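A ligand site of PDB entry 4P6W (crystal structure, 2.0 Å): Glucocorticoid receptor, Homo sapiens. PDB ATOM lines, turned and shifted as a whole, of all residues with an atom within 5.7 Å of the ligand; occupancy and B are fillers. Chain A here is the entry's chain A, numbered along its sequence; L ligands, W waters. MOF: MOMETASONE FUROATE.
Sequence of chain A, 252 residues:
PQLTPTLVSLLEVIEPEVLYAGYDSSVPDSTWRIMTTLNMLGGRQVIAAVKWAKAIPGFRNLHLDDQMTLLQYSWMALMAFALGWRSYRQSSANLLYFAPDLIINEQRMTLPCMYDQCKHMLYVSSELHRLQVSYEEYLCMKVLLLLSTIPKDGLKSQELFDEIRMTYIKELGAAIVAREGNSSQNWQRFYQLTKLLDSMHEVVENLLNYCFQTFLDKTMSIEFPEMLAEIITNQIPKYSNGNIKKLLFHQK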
ATOM      1  N   ILE A  34      12.205 -22.582   3.087  1.00  0.00           N
ATOM      2  CA  ILE A  34      11.130 -23.514   3.395  1.00  0.00           C
ATOM      3  C   ILE A  34       9.855 -22.787   3.828  1.00  0.00           C
ATOM      4  O   ILE A  34       8.765 -23.089   3.332  1.00  0.00           O
ATOM      5  CB  ILE A  34      11.558 -24.512   4.489  1.00  0.00           C
ATOM      6  CG1 ILE A  34      12.549 -25.518   3.898  1.00  0.00           C
ATOM      7  CG2 ILE A  34      10.350 -25.233   5.067  1.00  0.00           C
ATOM      8  CD1 ILE A  34      13.104 -26.483   4.902  1.00  0.00           C
ATOM      9  N   MET A  35       9.996 -21.836   4.736  1.00  0.00           N
ATOM     10  CA  MET A  35       8.850 -21.079   5.237  1.00  0.00           C
ATOM     11  C   MET A  35       8.148 -20.294   4.124  1.00  0.00           C
ATOM     12  O   MET A  35       6.920 -20.288   4.047  1.00  0.00           O
ATOM     13  CB  MET A  35       9.274 -20.134   6.354  1.00  0.00           C
ATOM     14  CG  MET A  35       9.672 -20.845   7.640  1.00  0.00           C
ATOM     15  SD  MET A  35      10.000 -19.715   8.998  1.00  0.00           S
ATOM     16  CE  MET A  35      10.124 -20.853  10.382  1.00  0.00           C
ATOM     17  N   LEU A  38       6.309 -22.683   1.891  1.00  0.00           N
ATOM     18  CA  LEU A  38       5.121 -23.214   2.566  1.00  0.00           C
ATOM     19  C   LEU A  38       4.013 -22.160   2.621  1.00  0.00           C
ATOM     20  O   LEU A  38       2.834 -22.490   2.477  1.00  0.00           O
ATOM     21  CB  LEU A  38       5.467 -23.702   3.967  1.00  0.00           C
ATOM     22  CG  LEU A  38       6.252 -25.025   3.985  1.00  0.00           C
ATOM     23  CD1 LEU A  38       6.675 -25.400   5.393  1.00  0.00           C
ATOM     24  CD2 LEU A  38       5.432 -26.125   3.348  1.00  0.00           C
ATOM     25  N   ASN A  39       4.389 -20.907   2.831  1.00  0.00           N
ATOM     26  CA  ASN A  39       3.428 -19.808   2.803  1.00  0.00           C
ATOM     27  C   ASN A  39       2.725 -19.694   1.456  1.00  0.00           C
ATOM     28  O   ASN A  39       1.510 -19.503   1.390  1.00  0.00           O
ATOM     29  CB  ASN A  39       4.099 -18.474   3.143  1.00  0.00           C
ATOM     30  CG  ASN A  39       4.244 -18.254   4.626  1.00  0.00           C
ATOM     31  OD1 ASN A  39       3.664 -18.981   5.432  1.00  0.00           O
ATOM     32  ND2 ASN A  39       5.013 -17.240   5.001  1.00  0.00           N
ATOM     33  N   LEU A  41       2.460 -22.125  -0.769  1.00  0.00           N
ATOM     34  CA  LEU A  41       1.650 -23.333  -0.860  1.00  0.00           C
ATOM     35  C   LEU A  41       0.357 -23.152  -0.066  1.00  0.00           C
ATOM     36  O   LEU A  41      -0.720 -23.510  -0.536  1.00  0.00           O
ATOM     37  CB  LEU A  41       2.413 -24.550  -0.358  1.00  0.00           C
ATOM     38  CG  LEU A  41       1.626 -25.851  -0.172  1.00  0.00           C
ATOM     39  CD1 LEU A  41       1.065 -26.362  -1.484  1.00  0.00           C
ATOM     40  CD2 LEU A  41       2.482 -26.917   0.505  1.00  0.00           C
ATOM     41  N   GLY A  42       0.480 -22.568   1.121  1.00  0.00           N
ATOM     42  CA  GLY A  42      -0.662 -22.325   1.987  1.00  0.00           C
ATOM     43  C   GLY A  42      -1.690 -21.425   1.342  1.00  0.00           C
ATOM     44  O   GLY A  42      -2.885 -21.696   1.416  1.00  0.00           O
ATOM     45  N   GLN A  45      -3.588 -23.479  -1.071  1.00  0.00           N
ATOM     46  CA  GLN A  45      -4.442 -24.446  -0.373  1.00  0.00           C
ATOM     47  C   GLN A  45      -5.690 -23.762   0.162  1.00  0.00           C
ATOM     48  O   GLN A  45      -6.785 -24.335   0.146  1.00  0.00           O
ATOM     49  CB  GLN A  45      -3.679 -25.126   0.761  1.00  0.00           C
ATOM     50  CG  GLN A  45      -2.613 -26.106   0.315  1.00  0.00           C
ATOM     51  CD  GLN A  45      -1.860 -26.686   1.496  1.00  0.00           C
ATOM     52  OE1 GLN A  45      -2.017 -26.252   2.631  1.00  0.00           O
ATOM     53  NE2 GLN A  45      -1.034 -27.686   1.223  1.00  0.00           N
ATOM     54  N   TRP A  75      -9.070 -20.852   8.743  1.00  0.00           N
ATOM     55  CA  TRP A  75      -8.153 -21.281   7.677  1.00  0.00           C
ATOM     56  C   TRP A  75      -6.964 -22.055   8.240  1.00  0.00           C
ATOM     57  O   TRP A  75      -6.563 -23.072   7.672  1.00  0.00           O
ATOM     58  CB  TRP A  75      -7.673 -20.080   6.852  1.00  0.00           C
ATOM     59  CG  TRP A  75      -6.677 -19.186   7.531  1.00  0.00           C
ATOM     60  CD1 TRP A  75      -6.937 -18.105   8.300  1.00  0.00           C
ATOM     61  CD2 TRP A  75      -5.248 -19.309   7.479  1.00  0.00           C
ATOM     62  NE1 TRP A  75      -5.767 -17.538   8.747  1.00  0.00           N
ATOM     63  CE2 TRP A  75      -4.714 -18.253   8.253  1.00  0.00           C
ATOM     64  CE3 TRP A  75      -4.369 -20.207   6.860  1.00  0.00           C
ATOM     65  CZ2 TRP A  75      -3.344 -18.083   8.418  1.00  0.00           C
ATOM     66  CZ3 TRP A  75      -3.006 -20.026   7.030  1.00  0.00           C
ATOM     67  CH2 TRP A  75      -2.515 -18.970   7.801  1.00  0.00           C
ATOM     68  N   MET A  76      -6.417 -21.608   9.361  1.00  0.00           N
ATOM     69  CA  MET A  76      -5.283 -22.299   9.985  1.00  0.00           C
ATOM     70  C   MET A  76      -5.711 -23.678  10.499  1.00  0.00           C
ATOM     71  O   MET A  76      -4.959 -24.651  10.367  1.00  0.00           O
ATOM     72  CB  MET A  76      -4.697 -21.463  11.126  1.00  0.00           C
ATOM     73  CG  MET A  76      -3.473 -22.099  11.783  1.00  0.00           C
ATOM     74  SD  MET A  76      -2.076 -22.313  10.635  1.00  0.00           S
ATOM     75  CE  MET A  76      -1.307 -20.690  10.773  1.00  0.00           C
ATOM     76  N   MET A  79      -6.002 -25.926   7.462  1.00  0.00           N
ATOM     77  CA  MET A  79      -4.697 -26.250   6.896  1.00  0.00           C
ATOM     78  C   MET A  79      -3.928 -27.227   7.781  1.00  0.00           C
ATOM     79  O   MET A  79      -3.356 -28.191   7.296  1.00  0.00           O
ATOM     80  CB  MET A  79      -3.878 -24.978   6.660  1.00  0.00           C
ATOM     81  CG  MET A  79      -4.464 -24.032   5.607  1.00  0.00           C
ATOM     82  SD  MET A  79      -4.814 -24.853   4.042  1.00  0.00           S
ATOM     83  CE  MET A  79      -6.590 -25.021   4.098  1.00  0.00           C
ATOM     84  N   ALA A  80      -3.926 -26.967   9.089  1.00  0.00           N
ATOM     85  CA  ALA A  80      -3.197 -27.823  10.029  1.00  0.00           C
ATOM     86  C   ALA A  80      -3.814 -29.223  10.122  1.00  0.00           C
ATOM     87  O   ALA A  80      -3.090 -30.208  10.271  1.00  0.00           O
ATOM     88  CB  ALA A  80      -3.144 -27.175  11.401  1.00  0.00           C
ATOM     89  N   LEU A  83      -2.903 -31.149   7.010  1.00  0.00           N
ATOM     90  CA  LEU A  83      -1.487 -31.491   7.154  1.00  0.00           C
ATOM     91  C   LEU A  83      -1.313 -32.705   8.051  1.00  0.00           C
ATOM     92  O   LEU A  83      -0.575 -33.642   7.724  1.00  0.00           O
ATOM     93  CB  LEU A  83      -0.697 -30.310   7.723  1.00  0.00           C
ATOM     94  CG  LEU A  83       0.740 -30.632   8.153  1.00  0.00           C
ATOM     95  CD1 LEU A  83       1.560 -31.122   6.969  1.00  0.00           C
ATOM     96  CD2 LEU A  83       1.389 -29.417   8.800  1.00  0.00           C
ATOM     97  N   ARG A  86      -2.481 -35.922   6.106  1.00  0.00           N
ATOM     98  CA  ARG A  86      -1.513 -36.387   5.123  1.00  0.00           C
ATOM     99  C   ARG A  86      -0.313 -37.047   5.818  1.00  0.00           C
ATOM    100  O   ARG A  86       0.185 -38.084   5.369  1.00  0.00           O
ATOM    101  CB  ARG A  86      -1.028 -35.238   4.236  1.00  0.00           C
ATOM    102  CG  ARG A  86      -2.096 -34.684   3.295  1.00  0.00           C
ATOM    103  CD  ARG A  86      -1.493 -33.744   2.260  1.00  0.00           C
ATOM    104  NE  ARG A  86      -0.806 -32.596   2.871  1.00  0.00           N
ATOM    105  CZ  ARG A  86      -1.410 -31.465   3.209  1.00  0.00           C
ATOM    106  NH1 ARG A  86      -2.716 -31.326   3.016  1.00  0.00           N
ATOM    107  NH2 ARG A  86      -0.725 -30.481   3.756  1.00  0.00           N
ATOM    108  N   LEU A  96       6.294 -34.561   8.763  1.00  0.00           N
ATOM    109  CA  LEU A  96       5.239 -33.659   8.302  1.00  0.00           C
ATOM    110  C   LEU A  96       5.216 -33.623   6.775  1.00  0.00           C
ATOM    111  O   LEU A  96       6.168 -33.175   6.132  1.00  0.00           O
ATOM    112  CB  LEU A  96       5.452 -32.268   8.885  1.00  0.00           C
ATOM    113  CG  LEU A  96       5.256 -32.154  10.391  1.00  0.00           C
ATOM    114  CD1 LEU A  96       5.659 -30.770  10.889  1.00  0.00           C
ATOM    115  CD2 LEU A  96       3.805 -32.442  10.760  1.00  0.00           C
ATOM    116  N   PHE A  98       3.888 -31.884   4.079  1.00  0.00           N
ATOM    117  CA  PHE A  98       3.259 -30.667   3.580  1.00  0.00           C
ATOM    118  C   PHE A  98       2.820 -30.847   2.132  1.00  0.00           C
ATOM    119  O   PHE A  98       1.763 -30.371   1.732  1.00  0.00           O
ATOM    120  CB  PHE A  98       4.202 -29.474   3.705  1.00  0.00           C
ATOM    121  CG  PHE A  98       4.586 -29.159   5.111  1.00  0.00           C
ATOM    122  CD1 PHE A  98       5.719 -29.711   5.660  1.00  0.00           C
ATOM    123  CD2 PHE A  98       3.810 -28.317   5.876  1.00  0.00           C
ATOM    124  CE1 PHE A  98       6.083 -29.435   6.955  1.00  0.00           C
ATOM    125  CE2 PHE A  98       4.160 -28.029   7.183  1.00  0.00           C
ATOM    126  CZ  PHE A  98       5.307 -28.583   7.719  1.00  0.00           C
ATOM    127  N   ILE A 104       9.050 -32.861   5.686  1.00  0.00           N
ATOM    128  CA  ILE A 104       9.985 -32.541   6.742  1.00  0.00           C
ATOM    129  C   ILE A 104      10.087 -33.685   7.744  1.00  0.00           C
ATOM    130  O   ILE A 104       9.160 -33.949   8.507  1.00  0.00           O
ATOM    131  CB  ILE A 104       9.586 -31.243   7.463  1.00  0.00           C
ATOM    132  CG1 ILE A 104       9.708 -30.065   6.486  1.00  0.00           C
ATOM    133  CG2 ILE A 104      10.459 -31.015   8.682  1.00  0.00           C
ATOM    134  CD1 ILE A 104       9.381 -28.727   7.096  1.00  0.00           C
ATOM    135  N   CYS A 113      14.741 -22.453  14.139  1.00  0.00           N
ATOM    136  CA  CYS A 113      13.382 -21.975  14.364  1.00  0.00           C
ATOM    137  C   CYS A 113      12.295 -22.934  13.884  1.00  0.00           C
ATOM    138  O   CYS A 113      11.171 -22.505  13.617  1.00  0.00           O
ATOM    139  CB  CYS A 113      13.162 -20.619  13.697  1.00  0.00           C
ATOM    140  SG  CYS A 113      14.156 -19.260  14.366  1.00  0.00           S
ATOM    141  N   MET A 114      12.599 -24.224  13.782  1.00  0.00           N
ATOM    142  CA  MET A 114      11.615 -25.156  13.233  1.00  0.00           C
ATOM    143  C   MET A 114      11.147 -26.255  14.177  1.00  0.00           C
ATOM    144  O   MET A 114      10.119 -26.890  13.925  1.00  0.00           O
ATOM    145  CB  MET A 114      12.165 -25.800  11.962  1.00  0.00           C
ATOM    146  CG  MET A 114      11.941 -24.962  10.717  1.00  0.00           C
ATOM    147  SD  MET A 114      12.318 -25.870   9.213  1.00  0.00           S
ATOM    148  CE  MET A 114      11.512 -27.426   9.566  1.00  0.00           C
ATOM    149  N   GLN A 117       7.653 -25.459  16.341  1.00  0.00           N
ATOM    150  CA  GLN A 117       6.514 -25.368  15.419  1.00  0.00           C
ATOM    151  C   GLN A 117       6.120 -26.737  14.898  1.00  0.00           C
ATOM    152  O   GLN A 117       4.938 -27.086  14.879  1.00  0.00           O
ATOM    153  CB  GLN A 117       6.836 -24.429  14.255  1.00  0.00           C
ATOM    154  CG  GLN A 117       6.679 -22.960  14.574  1.00  0.00           C
ATOM    155  CD  GLN A 117       7.608 -22.526  15.696  1.00  0.00           C
ATOM    156  OE1 GLN A 117       7.157 -22.196  16.800  1.00  0.00           O
ATOM    157  NE2 GLN A 117       8.905 -22.525  15.418  1.00  0.00           N
ATOM    158  N   CYS A 118       7.107 -27.495  14.442  1.00  0.00           N
ATOM    159  CA  CYS A 118       6.846 -28.824  13.917  1.00  0.00           C
ATOM    160  C   CYS A 118       6.235 -29.741  14.969  1.00  0.00           C
ATOM    161  O   CYS A 118       5.403 -30.590  14.662  1.00  0.00           O
ATOM    162  CB  CYS A 118       8.131 -29.450  13.366  1.00  0.00           C
ATOM    163  SG  CYS A 118       8.708 -28.691  11.821  1.00  0.00           S
ATOM    164  N   MET A 121       2.582 -29.054  15.239  1.00  0.00           N
ATOM    165  CA  MET A 121       1.911 -29.600  14.069  1.00  0.00           C
ATOM    166  C   MET A 121       1.844 -31.124  14.118  1.00  0.00           C
ATOM    167  O   MET A 121       0.865 -31.721  13.683  1.00  0.00           O
ATOM    168  CB  MET A 121       2.620 -29.152  12.783  1.00  0.00           C
ATOM    169  CG  MET A 121       2.363 -27.699  12.428  1.00  0.00           C
ATOM    170  SD  MET A 121       3.261 -27.151  10.972  1.00  0.00           S
ATOM    171  CE  MET A 121       4.670 -26.340  11.718  1.00  0.00           C
ATOM    172  N   LEU A 207       0.031 -21.986  16.508  1.00  0.00           N
ATOM    173  CA  LEU A 207       0.505 -21.783  15.146  1.00  0.00           C
ATOM    174  C   LEU A 207       0.278 -20.341  14.673  1.00  0.00           C
ATOM    175  O   LEU A 207       1.121 -19.771  13.972  1.00  0.00           O
ATOM    176  CB  LEU A 207      -0.164 -22.769  14.184  1.00  0.00           C
ATOM    177  CG  LEU A 207       0.100 -24.249  14.444  1.00  0.00           C
ATOM    178  CD1 LEU A 207      -0.653 -25.127  13.456  1.00  0.00           C
ATOM    179  CD2 LEU A 207       1.593 -24.552  14.406  1.00  0.00           C
ATOM    180  N   TYR A 210       2.795 -17.760  16.239  1.00  0.00           N
ATOM    181  CA  TYR A 210       4.086 -17.778  15.568  1.00  0.00           C
ATOM    182  C   TYR A 210       3.953 -17.203  14.153  1.00  0.00           C
ATOM    183  O   TYR A 210       4.856 -16.513  13.673  1.00  0.00           O
ATOM    184  CB  TYR A 210       4.662 -19.190  15.529  1.00  0.00           C
ATOM    185  CG  TYR A 210       6.093 -19.222  15.072  1.00  0.00           C
ATOM    186  CD1 TYR A 210       6.398 -19.189  13.714  1.00  0.00           C
ATOM    187  CD2 TYR A 210       7.145 -19.281  15.996  1.00  0.00           C
ATOM    188  CE1 TYR A 210       7.700 -19.239  13.264  1.00  0.00           C
ATOM    189  CE2 TYR A 210       8.453 -19.307  15.564  1.00  0.00           C
ATOM    190  CZ  TYR A 210       8.724 -19.266  14.195  1.00  0.00           C
ATOM    191  OH  TYR A 210      10.026 -19.305  13.744  1.00  0.00           O
ATOM    192  N   CYS A 211       2.840 -17.494  13.489  1.00  0.00           N
ATOM    193  CA  CYS A 211       2.573 -16.965  12.158  1.00  0.00           C
ATOM    194  C   CYS A 211       2.507 -15.436  12.186  1.00  0.00           C
ATOM    195  O   CYS A 211       3.117 -14.763  11.363  1.00  0.00           O
ATOM    196  CB  CYS A 211       1.271 -17.542  11.588  1.00  0.00           C
ATOM    197  SG  CYS A 211       0.775 -16.874   9.993  1.00  0.00           S
ATOM    198  N   THR A 214       5.992 -13.951  12.822  1.00  0.00           N
ATOM    199  CA  THR A 214       6.803 -13.996  11.623  1.00  0.00           C
ATOM    200  C   THR A 214       6.347 -12.942  10.611  1.00  0.00           C
ATOM    201  O   THR A 214       7.170 -12.266   9.991  1.00  0.00           O
ATOM    202  CB  THR A 214       6.751 -15.381  10.964  1.00  0.00           C
ATOM    203  OG1 THR A 214       7.198 -16.369  11.892  1.00  0.00           O
ATOM    204  CG2 THR A 214       7.643 -15.413   9.733  1.00  0.00           C
ATOM    205  N   ILE A 222      10.632 -13.211   5.080  1.00  0.00           N
ATOM    206  CA  ILE A 222       9.817 -14.342   4.672  1.00  0.00           C
ATOM    207  C   ILE A 222       8.578 -13.821   3.941  1.00  0.00           C
ATOM    208  O   ILE A 222       7.900 -12.918   4.422  1.00  0.00           O
ATOM    209  CB  ILE A 222       9.399 -15.212   5.882  1.00  0.00           C
ATOM    210  CG1 ILE A 222      10.645 -15.809   6.526  1.00  0.00           C
ATOM    211  CG2 ILE A 222       8.429 -16.305   5.456  1.00  0.00           C
ATOM    212  CD1 ILE A 222      10.388 -16.489   7.844  1.00  0.00           C
ATOM    213  N   PHE A 224       4.797 -13.807   2.117  1.00  0.00           N
ATOM    214  CA  PHE A 224       3.431 -14.305   2.219  1.00  0.00           C
ATOM    215  C   PHE A 224       2.679 -13.946   0.941  1.00  0.00           C
ATOM    216  O   PHE A 224       2.862 -12.853   0.408  1.00  0.00           O
ATOM    217  CB  PHE A 224       2.715 -13.721   3.431  1.00  0.00           C
ATOM    218  CG  PHE A 224       3.265 -14.160   4.766  1.00  0.00           C
ATOM    219  CD1 PHE A 224       4.477 -13.684   5.218  1.00  0.00           C
ATOM    220  CD2 PHE A 224       2.551 -15.029   5.565  1.00  0.00           C
ATOM    221  CE1 PHE A 224       4.992 -14.082   6.443  1.00  0.00           C
ATOM    222  CE2 PHE A 224       3.044 -15.435   6.797  1.00  0.00           C
ATOM    223  CZ  PHE A 224       4.265 -14.963   7.229  1.00  0.00           C
ATOM    224  N   LEU A 228      -2.968 -14.994   2.220  1.00  0.00           N
ATOM    225  CA  LEU A 228      -2.660 -15.123   3.633  1.00  0.00           C
ATOM    226  C   LEU A 228      -2.401 -13.753   4.274  1.00  0.00           C
ATOM    227  O   LEU A 228      -2.833 -13.511   5.402  1.00  0.00           O
ATOM    228  CB  LEU A 228      -1.445 -16.030   3.848  1.00  0.00           C
ATOM    229  CG  LEU A 228      -1.559 -17.483   3.376  1.00  0.00           C
ATOM    230  CD1 LEU A 228      -0.451 -18.320   3.980  1.00  0.00           C
ATOM    231  CD2 LEU A 228      -2.927 -18.065   3.694  1.00  0.00           C
HETATM  232  O35 MOF L   1       0.326 -27.314   4.202  1.00  0.00           O
HETATM  233  C34 MOF L   1       0.332 -26.185   4.731  1.00  0.00           C
HETATM  234  C33 MOF L   1       0.894 -25.101   4.055  1.00  0.00           C
HETATM  235  C32 MOF L   1      -0.077 -26.062   6.046  1.00  0.00           C
HETATM  236  C29 MOF L   1      -0.044 -24.843   6.683  1.00  0.00           C
HETATM  237  C26 MOF L   1      -0.504 -24.779   8.121  1.00  0.00           C
HETATM  238  C24 MOF L   1       0.502 -23.603   6.022  1.00  0.00           C
HETATM  239  C30 MOF L   1       0.985 -23.857   4.663  1.00  0.00           C
HETATM  240  C31 MOF L   1      -0.686 -22.649   5.909  1.00  0.00           C
HETATM  241  C19 MOF L   1       1.713 -23.187   6.888  1.00  0.00           C
HETATM  242 CL25 MOF L   1       2.886 -24.571   6.924  1.00  0.00          CL
HETATM  243  C15 MOF L   1       2.594 -22.059   6.300  1.00  0.00           C
HETATM  244  O21 MOF L   1       1.857 -20.915   5.841  1.00  0.00           O
HETATM  245  C14 MOF L   1       1.251 -22.938   8.336  1.00  0.00           C
HETATM  246  C20 MOF L   1       0.630 -24.194   8.958  1.00  0.00           C
HETATM  247  C6  MOF L   1       2.441 -22.542   9.196  1.00  0.00           C
HETATM  248  C9  MOF L   1       2.224 -22.279  10.682  1.00  0.00           C
HETATM  249  C3  MOF L   1       3.475 -21.499  11.076  1.00  0.00           C
HETATM  250  C10 MOF L   1       4.057 -22.215  12.282  1.00  0.00           C
HETATM  251  C2  MOF L   1       3.195 -21.317   8.690  1.00  0.00           C
HETATM  252  C7  MOF L   1       3.684 -21.623   7.268  1.00  0.00           C
HETATM  253  C8  MOF L   1       2.376 -20.009   8.758  1.00  0.00           C
HETATM  254  C1  MOF L   1       4.294 -21.290   9.760  1.00  0.00           C
HETATM  255  C5  MOF L   1       5.047 -19.975   9.656  1.00  0.00           C
HETATM  256  O13 MOF L   1       4.768 -19.001  10.500  1.00  0.00           O
HETATM  257  C12 MOF L   1       6.113 -19.637   8.624  1.00  0.00           C
HETATM  258 CL18 MOF L   1       5.846 -17.990   7.816  1.00  0.00          CL
HETATM  259  O4  MOF L   1       5.184 -22.391   9.488  1.00  0.00           O
HETATM  260  C11 MOF L   1       6.538 -22.710   9.990  1.00  0.00           C
HETATM  261  O17 MOF L   1       7.253 -21.941  10.642  1.00  0.00           O
HETATM  262  C16 MOF L   1       7.104 -24.024   9.703  1.00  0.00           C
HETATM  263  C22 MOF L   1       6.650 -25.107   9.011  1.00  0.00           C
HETATM  264  C27 MOF L   1       7.675 -26.012   9.110  1.00  0.00           C
HETATM  265  C28 MOF L   1       8.688 -25.472   9.860  1.00  0.00           C
HETATM  266  O23 MOF L   1       8.335 -24.205  10.237  1.00  0.00           O
HETATM  267  O   HOH W   1      -2.751 -28.328   4.470  1.00  0.00           O
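The side-chain amide oxygen (OE1) of Gln 45 lies close to the side-chain sulfur (SD) of Met 79, 3.4 Å away. The side-chain amide nitrogen of Gln 117 is in hydrogen-bond range of the backbone carbonyl oxygen of Cys 113 (2.9 Å). The side-chain hydroxyl (OG1) of Thr 214 is in hydrogen-bond range of the backbone carbonyl oxygen (O) of Tyr 210 (2.9 Å). The backbone carbonyl oxygen (O) of Met 114 lies within hydrogen-bond range of the side-chain sulfur (SG) of Cys 118, 3.1 Å away. The backbone carbonyl oxygen of Phe 98 lies within hydrogen-bond range of the guanidinium group of Arg 86. The side-chain hydroxyl (OH) of Tyr 210 lies close to the backbone carbonyl oxygen (O) of Cys 113, at 3.4 Å. The backbone NH of Ile 104 sits at hydrogen-bond distance from the backbone carbonyl oxygen of Leu 96 (2.9 Å).
An oxygen (O21) of the ligand sits at hydrogen-bond distance from the side-chain amide oxygen of Asn 39, 2.7 Å away. An oxygen (O35) of the ligand sits close to the side-chain amide oxygen (OE1) of Gln 45 (3.0 Å). The guanidinium group of Arg 86 sits at hydrogen-bond distance from an oxygen (O35) of the ligand, at 3.4 Å.
Met 35 touches the ligand (CE to O17, 3.1 Å). O of Leu 38 touches C30 of the ligand, at 3.2 Å. CA of Gly 42 touches C30 of the ligand (3.5 Å). CZ3 of Trp 75 touches C31 of the ligand, 3.7 Å away. Met 76 touches the ligand (SD to C20, 3.7 Å). Met 79 touches the ligand. Phe 98 touches the ligand (CE2 to CL25, 3.7 Å). Ile 104 touches the ligand. CG of Met 114 touches C28 of the ligand (3.4 Å). Gln 117 touches the ligand (CG to C10, 3.6 Å). Cys 118 touches the ligand. Met 121 touches the ligand. Tyr 210 touches the ligand (CD1 to O13, 3.6 Å). CA of Cys 211 touches O13 of the ligand (3.4 Å). Thr 214 touches the ligand. Ile 222 touches the ligand (CG2 to CL18, 3.9 Å). CZ of Phe 224 touches CL18 of the ligand (3.5 Å). Leu 228 touches the ligand. 21 residues have an atom within 4 Å of the ligand: Met 35, Leu 38, Asn 39, Gly 42, Gln 45, Trp 75, Met 76, Met 79, Arg 86, Phe 98, Ile 104, Met 114, Gln 117, Cys 118, Met 121, Tyr 210, Cys 211, Thr 214, Ile 222, Phe 224 and Leu 228. The nearest printed residue that does not touch the ligand is Leu 207 (4.01 Å).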
